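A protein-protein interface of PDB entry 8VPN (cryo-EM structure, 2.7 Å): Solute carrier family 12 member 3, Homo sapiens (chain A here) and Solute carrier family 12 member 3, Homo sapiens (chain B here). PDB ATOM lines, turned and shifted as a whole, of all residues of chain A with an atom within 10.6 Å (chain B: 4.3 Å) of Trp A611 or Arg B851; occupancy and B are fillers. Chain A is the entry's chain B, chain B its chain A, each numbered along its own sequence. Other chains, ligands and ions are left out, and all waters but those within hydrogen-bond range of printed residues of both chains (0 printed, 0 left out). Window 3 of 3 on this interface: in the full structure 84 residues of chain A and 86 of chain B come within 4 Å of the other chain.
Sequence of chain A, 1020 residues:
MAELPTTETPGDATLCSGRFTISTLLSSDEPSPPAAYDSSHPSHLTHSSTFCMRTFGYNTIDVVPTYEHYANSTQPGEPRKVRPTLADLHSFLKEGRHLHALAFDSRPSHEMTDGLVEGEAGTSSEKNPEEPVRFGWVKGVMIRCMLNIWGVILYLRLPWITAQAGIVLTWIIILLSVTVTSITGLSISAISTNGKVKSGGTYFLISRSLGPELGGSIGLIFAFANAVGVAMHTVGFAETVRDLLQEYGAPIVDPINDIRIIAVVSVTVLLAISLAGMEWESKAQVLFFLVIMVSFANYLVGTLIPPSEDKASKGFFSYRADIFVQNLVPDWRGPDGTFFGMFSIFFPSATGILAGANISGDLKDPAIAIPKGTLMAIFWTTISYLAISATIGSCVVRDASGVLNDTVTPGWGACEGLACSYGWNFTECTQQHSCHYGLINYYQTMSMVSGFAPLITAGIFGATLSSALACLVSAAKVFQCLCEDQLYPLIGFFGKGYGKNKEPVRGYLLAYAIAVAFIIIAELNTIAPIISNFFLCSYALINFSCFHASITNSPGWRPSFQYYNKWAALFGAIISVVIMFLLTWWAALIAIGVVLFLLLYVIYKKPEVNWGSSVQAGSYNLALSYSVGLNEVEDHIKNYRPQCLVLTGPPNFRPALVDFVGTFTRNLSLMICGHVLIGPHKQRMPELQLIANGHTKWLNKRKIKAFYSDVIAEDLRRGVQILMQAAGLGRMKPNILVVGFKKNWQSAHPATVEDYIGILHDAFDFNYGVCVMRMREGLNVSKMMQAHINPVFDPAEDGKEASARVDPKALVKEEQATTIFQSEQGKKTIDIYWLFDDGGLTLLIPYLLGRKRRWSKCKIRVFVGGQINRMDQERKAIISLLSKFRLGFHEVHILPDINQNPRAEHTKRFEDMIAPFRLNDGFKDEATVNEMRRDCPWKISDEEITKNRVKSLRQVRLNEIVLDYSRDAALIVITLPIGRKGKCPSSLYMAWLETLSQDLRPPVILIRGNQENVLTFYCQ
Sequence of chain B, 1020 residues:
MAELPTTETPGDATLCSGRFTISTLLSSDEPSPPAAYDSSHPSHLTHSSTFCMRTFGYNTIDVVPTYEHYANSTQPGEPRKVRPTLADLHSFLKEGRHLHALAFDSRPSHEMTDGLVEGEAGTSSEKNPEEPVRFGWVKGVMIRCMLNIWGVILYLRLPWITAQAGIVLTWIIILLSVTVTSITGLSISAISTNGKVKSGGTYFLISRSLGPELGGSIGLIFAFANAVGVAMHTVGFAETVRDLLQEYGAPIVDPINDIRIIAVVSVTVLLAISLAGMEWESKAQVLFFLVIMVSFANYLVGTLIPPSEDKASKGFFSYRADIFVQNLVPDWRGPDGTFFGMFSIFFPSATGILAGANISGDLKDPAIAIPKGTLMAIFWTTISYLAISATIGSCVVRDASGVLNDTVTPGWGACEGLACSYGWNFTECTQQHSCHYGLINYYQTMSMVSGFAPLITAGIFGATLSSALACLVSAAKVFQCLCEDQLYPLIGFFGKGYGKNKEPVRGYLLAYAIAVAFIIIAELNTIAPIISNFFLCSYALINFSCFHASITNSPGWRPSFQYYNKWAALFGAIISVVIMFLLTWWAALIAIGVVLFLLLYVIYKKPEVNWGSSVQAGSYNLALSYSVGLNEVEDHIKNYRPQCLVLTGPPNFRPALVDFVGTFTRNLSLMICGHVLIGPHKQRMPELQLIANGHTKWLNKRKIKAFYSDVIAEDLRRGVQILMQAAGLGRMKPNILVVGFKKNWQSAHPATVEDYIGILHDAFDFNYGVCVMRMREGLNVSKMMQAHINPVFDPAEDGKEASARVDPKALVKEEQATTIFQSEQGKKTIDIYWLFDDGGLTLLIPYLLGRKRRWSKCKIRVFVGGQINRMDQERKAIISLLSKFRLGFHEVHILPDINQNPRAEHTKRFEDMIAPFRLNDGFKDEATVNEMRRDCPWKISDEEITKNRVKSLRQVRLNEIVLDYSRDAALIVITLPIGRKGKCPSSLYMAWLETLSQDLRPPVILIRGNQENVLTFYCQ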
ATOM      1  N   PHE A 204      28.104 -21.962   9.973  1.00  0.00           N
ATOM      2  CA  PHE A 204      26.756 -22.468   9.751  1.00  0.00           C
ATOM      3  C   PHE A 204      25.757 -21.794  10.682  1.00  0.00           C
ATOM      4  O   PHE A 204      24.661 -21.408  10.257  1.00  0.00           O
ATOM      5  CB  PHE A 204      26.734 -23.986   9.939  1.00  0.00           C
ATOM      6  N   SER A 207      25.155 -18.144   9.572  1.00  0.00           N
ATOM      7  CA  SER A 207      24.349 -18.097   8.357  1.00  0.00           C
ATOM      8  C   SER A 207      22.892 -18.426   8.652  1.00  0.00           C
ATOM      9  O   SER A 207      21.982 -17.746   8.160  1.00  0.00           O
ATOM     10  CB  SER A 207      24.915 -19.059   7.313  1.00  0.00           C
ATOM     11  N   ARG A 208      22.652 -19.457   9.464  1.00  0.00           N
ATOM     12  CA  ARG A 208      21.285 -19.845   9.791  1.00  0.00           C
ATOM     13  C   ARG A 208      20.567 -18.765  10.589  1.00  0.00           C
ATOM     14  O   ARG A 208      19.339 -18.650  10.502  1.00  0.00           O
ATOM     15  CB  ARG A 208      21.285 -21.163  10.565  1.00  0.00           C
ATOM     16  N   SER A 209      21.300 -17.978  11.376  1.00  0.00           N
ATOM     17  CA  SER A 209      20.659 -16.939  12.179  1.00  0.00           C
ATOM     18  C   SER A 209      20.406 -15.654  11.393  1.00  0.00           C
ATOM     19  O   SER A 209      19.312 -15.089  11.469  1.00  0.00           O
ATOM     20  CB  SER A 209      21.502 -16.635  13.422  1.00  0.00           C
ATOM     21  N   GLY A 211      20.837 -15.248   7.945  1.00  0.00           N
ATOM     22  CA  GLY A 211      20.660 -15.464   6.527  1.00  0.00           C
ATOM     23  C   GLY A 211      21.977 -15.657   5.801  1.00  0.00           C
ATOM     24  O   GLY A 211      23.057 -15.588   6.395  1.00  0.00           O
ATOM     25  N   PRO A 212      21.912 -15.911   4.491  1.00  0.00           N
ATOM     26  CA  PRO A 212      23.146 -16.128   3.723  1.00  0.00           C
ATOM     27  C   PRO A 212      23.785 -14.848   3.206  1.00  0.00           C
ATOM     28  O   PRO A 212      25.006 -14.794   3.016  1.00  0.00           O
ATOM     29  CB  PRO A 212      22.681 -17.023   2.568  1.00  0.00           C
ATOM     30  N   LEU A 482      32.091 -24.957   4.192  1.00  0.00           N
ATOM     31  CA  LEU A 482      31.642 -24.396   2.924  1.00  0.00           C
ATOM     32  C   LEU A 482      31.415 -25.499   1.898  1.00  0.00           C
ATOM     33  O   LEU A 482      30.381 -25.527   1.220  1.00  0.00           O
ATOM     34  CB  LEU A 482      32.662 -23.381   2.406  1.00  0.00           C
ATOM     35  N   ASP A 485      29.025 -30.281   2.363  1.00  0.00           N
ATOM     36  CA  ASP A 485      27.891 -31.040   1.846  1.00  0.00           C
ATOM     37  C   ASP A 485      28.199 -31.709   0.511  1.00  0.00           C
ATOM     38  O   ASP A 485      28.258 -32.935   0.423  1.00  0.00           O
ATOM     39  CB  ASP A 485      26.668 -30.130   1.708  1.00  0.00           C
ATOM     40  N   LYS A 606      23.435 -16.916  -9.360  1.00  0.00           N
ATOM     41  CA  LYS A 606      22.372 -17.607 -10.089  1.00  0.00           C
ATOM     42  C   LYS A 606      21.985 -18.885  -9.350  1.00  0.00           C
ATOM     43  O   LYS A 606      20.924 -18.930  -8.712  1.00  0.00           O
ATOM     44  CB  LYS A 606      22.774 -17.912 -11.536  1.00  0.00           C
ATOM     45  N   PRO A 607      22.807 -19.942  -9.400  1.00  0.00           N
ATOM     46  CA  PRO A 607      22.468 -21.162  -8.659  1.00  0.00           C
ATOM     47  C   PRO A 607      22.882 -21.053  -7.203  1.00  0.00           C
ATOM     48  O   PRO A 607      23.981 -21.477  -6.832  1.00  0.00           O
ATOM     49  CB  PRO A 607      23.257 -22.249  -9.396  1.00  0.00           C
ATOM     50  CG  PRO A 607      24.410 -21.522 -10.043  1.00  0.00           C
ATOM     51  CD  PRO A 607      24.152 -20.033  -9.988  1.00  0.00           C
ATOM     52  N   GLU A 608      22.019 -20.465  -6.373  1.00  0.00           N
ATOM     53  CA  GLU A 608      22.378 -20.138  -5.000  1.00  0.00           C
ATOM     54  C   GLU A 608      22.309 -21.327  -4.052  1.00  0.00           C
ATOM     55  O   GLU A 608      22.703 -21.188  -2.890  1.00  0.00           O
ATOM     56  CB  GLU A 608      21.474 -19.018  -4.478  1.00  0.00           C
ATOM     57  N   VAL A 609      21.830 -22.482  -4.506  1.00  0.00           N
ATOM     58  CA  VAL A 609      21.657 -23.630  -3.623  1.00  0.00           C
ATOM     59  C   VAL A 609      22.769 -24.645  -3.852  1.00  0.00           C
ATOM     60  O   VAL A 609      23.536 -24.958  -2.935  1.00  0.00           O
ATOM     61  CB  VAL A 609      20.278 -24.278  -3.825  1.00  0.00           C
ATOM     62  N   ASN A 610      22.873 -25.155  -5.079  1.00  0.00           N
ATOM     63  CA  ASN A 610      23.849 -26.191  -5.416  1.00  0.00           C
ATOM     64  C   ASN A 610      23.524 -27.520  -4.729  1.00  0.00           C
ATOM     65  O   ASN A 610      24.369 -28.120  -4.065  1.00  0.00           O
ATOM     66  CB  ASN A 610      25.267 -25.734  -5.070  1.00  0.00           C
ATOM     67  N   TRP A 611      22.290 -27.983  -4.905  1.00  0.00           N
ATOM     68  CA  TRP A 611      21.885 -29.263  -4.343  1.00  0.00           C
ATOM     69  C   TRP A 611      22.577 -30.421  -5.058  1.00  0.00           C
ATOM     70  O   TRP A 611      23.004 -30.303  -6.209  1.00  0.00           O
ATOM     71  CB  TRP A 611      20.373 -29.448  -4.452  1.00  0.00           C
ATOM     72  CG  TRP A 611      19.543 -28.361  -3.834  1.00  0.00           C
ATOM     73  CD1 TRP A 611      19.099 -27.231  -4.446  1.00  0.00           C
ATOM     74  CD2 TRP A 611      19.035 -28.318  -2.494  1.00  0.00           C
ATOM     75  NE1 TRP A 611      18.354 -26.477  -3.571  1.00  0.00           N
ATOM     76  CE2 TRP A 611      18.301 -27.123  -2.365  1.00  0.00           C
ATOM     77  CE3 TRP A 611      19.137 -29.168  -1.392  1.00  0.00           C
ATOM     78  CZ2 TRP A 611      17.669 -26.758  -1.180  1.00  0.00           C
ATOM     79  CZ3 TRP A 611      18.508 -28.805  -0.215  1.00  0.00           C
ATOM     80  CH2 TRP A 611      17.785 -27.608  -0.118  1.00  0.00           C
ATOM     81  N   GLY A 612      22.682 -31.549  -4.356  1.00  0.00           N
ATOM     82  CA  GLY A 612      23.096 -32.814  -4.937  1.00  0.00           C
ATOM     83  C   GLY A 612      24.235 -32.747  -5.933  1.00  0.00           C
ATOM     84  O   GLY A 612      24.021 -32.961  -7.129  1.00  0.00           O
ATOM     85  N   SER A 613      25.449 -32.470  -5.460  1.00  0.00           N
ATOM     86  CA  SER A 613      26.571 -32.234  -6.360  1.00  0.00           C
ATOM     87  C   SER A 613      26.746 -33.378  -7.352  1.00  0.00           C
ATOM     88  O   SER A 613      27.084 -34.507  -6.974  1.00  0.00           O
ATOM     89  CB  SER A 613      27.856 -32.013  -5.560  1.00  0.00           C
ATOM     90  OG  SER A 613      27.594 -31.284  -4.374  1.00  0.00           O
ATOM     91  N   SER A 614      26.513 -33.087  -8.625  1.00  0.00           N
ATOM     92  CA  SER A 614      26.606 -34.056  -9.713  1.00  0.00           C
ATOM     93  C   SER A 614      26.526 -33.275 -11.022  1.00  0.00           C
ATOM     94  O   SER A 614      26.542 -32.038 -11.027  1.00  0.00           O
ATOM     95  CB  SER A 614      25.514 -35.119  -9.603  1.00  0.00           C
ATOM     96  OG  SER A 614      24.261 -34.598 -10.008  1.00  0.00           O
ATOM     97  N   VAL A 615      26.444 -33.997 -12.138  1.00  0.00           N
ATOM     98  CA  VAL A 615      26.308 -33.348 -13.440  1.00  0.00           C
ATOM     99  C   VAL A 615      24.856 -32.962 -13.694  1.00  0.00           C
ATOM    100  O   VAL A 615      24.532 -31.787 -13.911  1.00  0.00           O
ATOM    101  CB  VAL A 615      26.848 -34.265 -14.551  1.00  0.00           C
ATOM    102  CG1 VAL A 615      28.371 -34.293 -14.523  1.00  0.00           C
ATOM    103  CG2 VAL A 615      26.290 -35.666 -14.392  1.00  0.00           C
ATOM    104  N   GLN A 616      23.963 -33.952 -13.669  1.00  0.00           N
ATOM    105  CA  GLN A 616      22.543 -33.692 -13.875  1.00  0.00           C
ATOM    106  C   GLN A 616      22.033 -32.613 -12.929  1.00  0.00           C
ATOM    107  O   GLN A 616      21.258 -31.737 -13.329  1.00  0.00           O
ATOM    108  CB  GLN A 616      21.753 -34.991 -13.688  1.00  0.00           C
ATOM    109  CG  GLN A 616      20.254 -34.851 -13.852  1.00  0.00           C
ATOM    110  CD  GLN A 616      19.689 -35.770 -14.918  1.00  0.00           C
ATOM    111  OE1 GLN A 616      19.755 -36.994 -14.797  1.00  0.00           O
ATOM    112  NE2 GLN A 616      19.126 -35.186 -15.969  1.00  0.00           N
ATOM    113  N   ALA A 617      22.462 -32.659 -11.666  1.00  0.00           N
ATOM    114  CA  ALA A 617      21.962 -31.710 -10.676  1.00  0.00           C
ATOM    115  C   ALA A 617      22.366 -30.280 -11.019  1.00  0.00           C
ATOM    116  O   ALA A 617      21.531 -29.367 -11.008  1.00  0.00           O
ATOM    117  CB  ALA A 617      22.467 -32.095  -9.288  1.00  0.00           C
ATOM    118  N   GLY A 618      23.646 -30.064 -11.330  1.00  0.00           N
ATOM    119  CA  GLY A 618      24.088 -28.725 -11.688  1.00  0.00           C
ATOM    120  C   GLY A 618      23.444 -28.224 -12.964  1.00  0.00           C
ATOM    121  O   GLY A 618      23.064 -27.051 -13.067  1.00  0.00           O
ATOM    122  N   SER A 619      23.315 -29.105 -13.958  1.00  0.00           N
ATOM    123  CA  SER A 619      22.646 -28.724 -15.196  1.00  0.00           C
ATOM    124  C   SER A 619      21.217 -28.274 -14.922  1.00  0.00           C
ATOM    125  O   SER A 619      20.777 -27.221 -15.406  1.00  0.00           O
ATOM    126  CB  SER A 619      22.665 -29.898 -16.171  1.00  0.00           C
ATOM    127  OG  SER A 619      21.930 -30.987 -15.644  1.00  0.00           O
ATOM    128  N   TYR A 620      20.482 -29.055 -14.129  1.00  0.00           N
ATOM    129  CA  TYR A 620      19.108 -28.700 -13.805  1.00  0.00           C
ATOM    130  C   TYR A 620      19.048 -27.372 -13.062  1.00  0.00           C
ATOM    131  O   TYR A 620      18.170 -26.541 -13.327  1.00  0.00           O
ATOM    132  CB  TYR A 620      18.463 -29.817 -12.984  1.00  0.00           C
ATOM    133  CG  TYR A 620      16.988 -29.627 -12.725  1.00  0.00           C
ATOM    134  CD1 TYR A 620      16.546 -28.779 -11.723  1.00  0.00           C
ATOM    135  CD2 TYR A 620      16.038 -30.291 -13.485  1.00  0.00           C
ATOM    136  CE1 TYR A 620      15.201 -28.596 -11.482  1.00  0.00           C
ATOM    137  CE2 TYR A 620      14.691 -30.116 -13.250  1.00  0.00           C
ATOM    138  CZ  TYR A 620      14.279 -29.268 -12.245  1.00  0.00           C
ATOM    139  OH  TYR A 620      12.938 -29.087 -12.008  1.00  0.00           O
ATOM    140  N   ASN A 621      19.978 -27.153 -12.131  1.00  0.00           N
ATOM    141  CA  ASN A 621      19.974 -25.912 -11.362  1.00  0.00           C
ATOM    142  C   ASN A 621      20.158 -24.706 -12.272  1.00  0.00           C
ATOM    143  O   ASN A 621      19.419 -23.718 -12.175  1.00  0.00           O
ATOM    144  CB  ASN A 621      21.073 -25.949 -10.305  1.00  0.00           C
ATOM    145  CG  ASN A 621      20.716 -26.825  -9.130  1.00  0.00           C
ATOM    146  OD1 ASN A 621      21.409 -27.799  -8.839  1.00  0.00           O
ATOM    147  ND2 ASN A 621      19.618 -26.503  -8.463  1.00  0.00           N
ATOM    148  N   LEU A 622      21.149 -24.769 -13.164  1.00  0.00           N
ATOM    149  CA  LEU A 622      21.389 -23.646 -14.065  1.00  0.00           C
ATOM    150  C   LEU A 622      20.196 -23.412 -14.983  1.00  0.00           C
ATOM    151  O   LEU A 622      19.784 -22.261 -15.209  1.00  0.00           O
ATOM    152  CB  LEU A 622      22.654 -23.892 -14.884  1.00  0.00           C
ATOM    153  CG  LEU A 622      23.985 -23.699 -14.165  1.00  0.00           C
ATOM    154  CD1 LEU A 622      25.064 -24.489 -14.865  1.00  0.00           C
ATOM    155  CD2 LEU A 622      24.351 -22.231 -14.101  1.00  0.00           C
ATOM    156  N   LEU A 624      17.010 -24.106 -14.502  1.00  0.00           N
ATOM    157  CA  LEU A 624      15.932 -23.473 -13.754  1.00  0.00           C
ATOM    158  C   LEU A 624      16.242 -22.010 -13.483  1.00  0.00           C
ATOM    159  O   LEU A 624      15.384 -21.137 -13.668  1.00  0.00           O
ATOM    160  CB  LEU A 624      15.685 -24.222 -12.446  1.00  0.00           C
ATOM    161  CG  LEU A 624      14.378 -23.896 -11.725  1.00  0.00           C
ATOM    162  CD1 LEU A 624      13.182 -24.463 -12.473  1.00  0.00           C
ATOM    163  CD2 LEU A 624      14.418 -24.417 -10.302  1.00  0.00           C
ATOM    164  N   SER A 625      17.469 -21.716 -13.047  1.00  0.00           N
ATOM    165  CA  SER A 625      17.803 -20.342 -12.691  1.00  0.00           C
ATOM    166  C   SER A 625      17.577 -19.407 -13.870  1.00  0.00           C
ATOM    167  O   SER A 625      16.875 -18.395 -13.748  1.00  0.00           O
ATOM    168  CB  SER A 625      19.248 -20.257 -12.197  1.00  0.00           C
ATOM    169  OG  SER A 625      20.145 -20.854 -13.112  1.00  0.00           O
ATOM    170  N   ARG B 641      13.025 -34.417  -8.107  1.00  0.00           N
ATOM    171  CA  ARG B 641      12.634 -33.141  -7.538  1.00  0.00           C
ATOM    172  C   ARG B 641      11.124 -33.019  -7.618  1.00  0.00           C
ATOM    173  O   ARG B 641      10.524 -33.488  -8.594  1.00  0.00           O
ATOM    174  CB  ARG B 641      13.283 -31.953  -8.252  1.00  0.00           C
ATOM    175  CG  ARG B 641      14.691 -32.199  -8.725  1.00  0.00           C
ATOM    176  CD  ARG B 641      15.653 -31.262  -8.028  1.00  0.00           C
ATOM    177  NE  ARG B 641      17.021 -31.446  -8.490  1.00  0.00           N
ATOM    178  CZ  ARG B 641      17.993 -30.564  -8.305  1.00  0.00           C
ATOM    179  NH1 ARG B 641      17.778 -29.424  -7.670  1.00  0.00           N
ATOM    180  NH2 ARG B 641      19.208 -30.831  -8.773  1.00  0.00           N
ATOM    181  N   ASN B 667      13.698 -21.802  -5.390  1.00  0.00           N
ATOM    182  CA  ASN B 667      15.109 -22.122  -5.595  1.00  0.00           C
ATOM    183  C   ASN B 667      15.379 -23.612  -5.740  1.00  0.00           C
ATOM    184  O   ASN B 667      16.545 -24.017  -5.740  1.00  0.00           O
ATOM    185  CB  ASN B 667      15.989 -21.583  -4.463  1.00  0.00           C
ATOM    186  CG  ASN B 667      16.319 -20.119  -4.628  1.00  0.00           C
ATOM    187  OD1 ASN B 667      16.282 -19.583  -5.733  1.00  0.00           O
ATOM    188  ND2 ASN B 667      16.650 -19.460  -3.523  1.00  0.00           N
ATOM    189  N   LEU B 668      14.354 -24.437  -5.844  1.00  0.00           N
ATOM    190  CA  LEU B 668      14.600 -25.874  -5.833  1.00  0.00           C
ATOM    191  C   LEU B 668      13.960 -26.625  -6.989  1.00  0.00           C
ATOM    192  O   LEU B 668      14.556 -27.582  -7.490  1.00  0.00           O
ATOM    193  CB  LEU B 668      14.115 -26.466  -4.510  1.00  0.00           C
ATOM    194  CG  LEU B 668      13.884 -27.969  -4.561  1.00  0.00           C
ATOM    195  CD1 LEU B 668      15.210 -28.657  -4.702  1.00  0.00           C
ATOM    196  CD2 LEU B 668      13.172 -28.429  -3.306  1.00  0.00           C
ATOM    197  N   TYR B 847       9.253 -31.990   5.732  1.00  0.00           N
ATOM    198  CA  TYR B 847      10.665 -31.812   6.055  1.00  0.00           C
ATOM    199  C   TYR B 847      11.243 -30.578   5.370  1.00  0.00           C
ATOM    200  O   TYR B 847      11.946 -29.780   5.999  1.00  0.00           O
ATOM    201  CB  TYR B 847      11.455 -33.059   5.663  1.00  0.00           C
ATOM    202  CG  TYR B 847      12.906 -32.776   5.377  1.00  0.00           C
ATOM    203  CD1 TYR B 847      13.784 -32.458   6.400  1.00  0.00           C
ATOM    204  CD2 TYR B 847      13.399 -32.813   4.082  1.00  0.00           C
ATOM    205  CE1 TYR B 847      15.111 -32.196   6.146  1.00  0.00           C
ATOM    206  CE2 TYR B 847      14.724 -32.549   3.816  1.00  0.00           C
ATOM    207  CZ  TYR B 847      15.576 -32.242   4.854  1.00  0.00           C
ATOM    208  OH  TYR B 847      16.899 -31.976   4.602  1.00  0.00           O
ATOM    209  N   LEU B 848      10.971 -30.411   4.076  1.00  0.00           N
ATOM    210  CA  LEU B 848      11.482 -29.247   3.360  1.00  0.00           C
ATOM    211  C   LEU B 848      10.870 -27.948   3.863  1.00  0.00           C
ATOM    212  O   LEU B 848      11.466 -26.883   3.672  1.00  0.00           O
ATOM    213  CB  LEU B 848      11.230 -29.396   1.860  1.00  0.00           C
ATOM    214  CG  LEU B 848      11.833 -30.631   1.182  1.00  0.00           C
ATOM    215  CD1 LEU B 848      10.952 -31.089   0.039  1.00  0.00           C
ATOM    216  CD2 LEU B 848      13.237 -30.346   0.688  1.00  0.00           C
ATOM    217  N   LEU B 849       9.698 -28.009   4.489  1.00  0.00           N
ATOM    218  CA  LEU B 849       9.064 -26.831   5.066  1.00  0.00           C
ATOM    219  C   LEU B 849       9.659 -26.449   6.415  1.00  0.00           C
ATOM    220  O   LEU B 849       9.275 -25.416   6.971  1.00  0.00           O
ATOM    221  CB  LEU B 849       7.556 -27.064   5.212  1.00  0.00           C
ATOM    222  CG  LEU B 849       6.641 -25.837   5.271  1.00  0.00           C
ATOM    223  CD1 LEU B 849       6.845 -24.958   4.055  1.00  0.00           C
ATOM    224  CD2 LEU B 849       5.181 -26.241   5.400  1.00  0.00           C
ATOM    225  N   GLY B 850      10.571 -27.259   6.954  1.00  0.00           N
ATOM    226  CA  GLY B 850      11.218 -26.986   8.221  1.00  0.00           C
ATOM    227  C   GLY B 850      12.670 -26.579   8.142  1.00  0.00           C
ATOM    228  O   GLY B 850      13.356 -26.597   9.171  1.00  0.00           O
ATOM    229  N   ARG B 851      13.179 -26.231   6.964  1.00  0.00           N
ATOM    230  CA  ARG B 851      14.510 -25.659   6.838  1.00  0.00           C
ATOM    231  C   ARG B 851      14.477 -24.145   6.698  1.00  0.00           C
ATOM    232  O   ARG B 851      15.521 -23.535   6.449  1.00  0.00           O
ATOM    233  CB  ARG B 851      15.243 -26.272   5.647  1.00  0.00           C
ATOM    234  CG  ARG B 851      15.306 -27.785   5.656  1.00  0.00           C
ATOM    235  CD  ARG B 851      16.038 -28.283   4.423  1.00  0.00           C
ATOM    236  NE  ARG B 851      17.067 -27.340   4.001  1.00  0.00           N
ATOM    237  CZ  ARG B 851      18.348 -27.646   3.843  1.00  0.00           C
ATOM    238  NH1 ARG B 851      18.799 -28.869   4.069  1.00  0.00           N
ATOM    239  NH2 ARG B 851      19.197 -26.703   3.447  1.00  0.00           N
ATOM    240  N   LYS B 852      13.311 -23.530   6.857  1.00  0.00           N
ATOM    241  CA  LYS B 852      13.140 -22.104   6.630  1.00  0.00           C
ATOM    242  C   LYS B 852      13.239 -21.329   7.939  1.00  0.00           C
ATOM    243  O   LYS B 852      13.258 -21.895   9.032  1.00  0.00           O
ATOM    244  CB  LYS B 852      11.798 -21.833   5.945  1.00  0.00           C
ATOM    245  CG  LYS B 852      11.690 -22.452   4.568  1.00  0.00           C
ATOM    246  CD  LYS B 852      12.953 -22.196   3.772  1.00  0.00           C
ATOM    247  CE  LYS B 852      12.842 -22.738   2.363  1.00  0.00           C
ATOM    248  NZ  LYS B 852      13.481 -21.815   1.384  1.00  0.00           N
ATOM    249  N   PHE B1017      17.029 -37.308  -3.766  1.00  0.00           N
ATOM    250  CA  PHE B1017      17.129 -35.867  -3.673  1.00  0.00           C
ATOM    251  C   PHE B1017      18.304 -35.399  -2.812  1.00  0.00           C
ATOM    252  O   PHE B1017      18.986 -34.449  -3.181  1.00  0.00           O
ATOM    253  CB  PHE B1017      15.816 -35.340  -3.106  1.00  0.00           C
ATOM    254  CG  PHE B1017      15.900 -33.957  -2.570  1.00  0.00           C
ATOM    255  CD1 PHE B1017      16.220 -33.740  -1.251  1.00  0.00           C
ATOM    256  CD2 PHE B1017      15.651 -32.877  -3.382  1.00  0.00           C
ATOM    257  CE1 PHE B1017      16.301 -32.465  -0.750  1.00  0.00           C
ATOM    258  CE2 PHE B1017      15.728 -31.596  -2.890  1.00  0.00           C
ATOM    259  CZ  PHE B1017      16.055 -31.391  -1.570  1.00  0.00           C
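Hydrophobic or aromatic side chains of chain B that line the printed part of chain A: Leu B668 and Phe B1017. Of the 27 printed residues of chain A, 3 touch a printed residue of chain B. Along chain A the printed residues that touch a printed residue of chain B span positions 611 to 621. Among the printed residues, 6 pairs touch across the chains. Among the printed residues, no Asp or Glu carboxylate lies within 4 Å of a Lys or Arg side-chain nitrogen of the other chain.
Among the printed residues, merely in contact across the chains: Ala A617 with Arg B641 (3.5 Å), Asn A621 with Arg B641 (3.5 Å), Trp A611 with Asn B667 (3.7 Å), Trp A611 with Phe B1017 (3.8 Å), Trp A611 with Arg B851 (3.9 Å) and Trp A611 with Leu B668 (3.99 Å).
Of the printed residues of chain B, Trp A611 touches Asn B667 (3.7 Å), Leu B668 (3.99 Å), Arg B851 (3.9 Å) and Phe B1017 (3.8 Å). Printed residues of chain B within 4 Å of Ala A617: Arg B641 (3.5 Å). Printed residues of chain B within 4 Å of Asn A621: Arg B641 (3.5 Å). Printed residues of chain A within 4 Å of Arg B641: Ala A617 (3.5 Å) and Asn A621 (3.5 Å). Printed residues of chain A within 4 Å of Asn B667: Trp A611. No residue of chain A comes within 4 Å of Gly B850. Of chain A, only Trp A611 (3.9 Å) comes within 4 Å of Arg B851. No residue of chain A comes within 4 Å of Lys B852. The nearest printed residue of chain B that does not touch Trp A611 is Arg B641 (4.1 Å). The nearest residue of chain A that does not touch Arg B851 is Arg A208 (7.4 Å).
The side-chain hydroxyl (OG) of Ser A614 lies within hydrogen-bond range of the backbone NH (N) of Ala A617 (3.1 Å). OG of Ser A625 sits at hydrogen-bond distance from O of Asn A621 (3.1 Å). The backbone carbonyl oxygen (O) of Ala A617 lies close to the side-chain amide oxygen (OD1) of Asn A621, 2.7 Å away.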
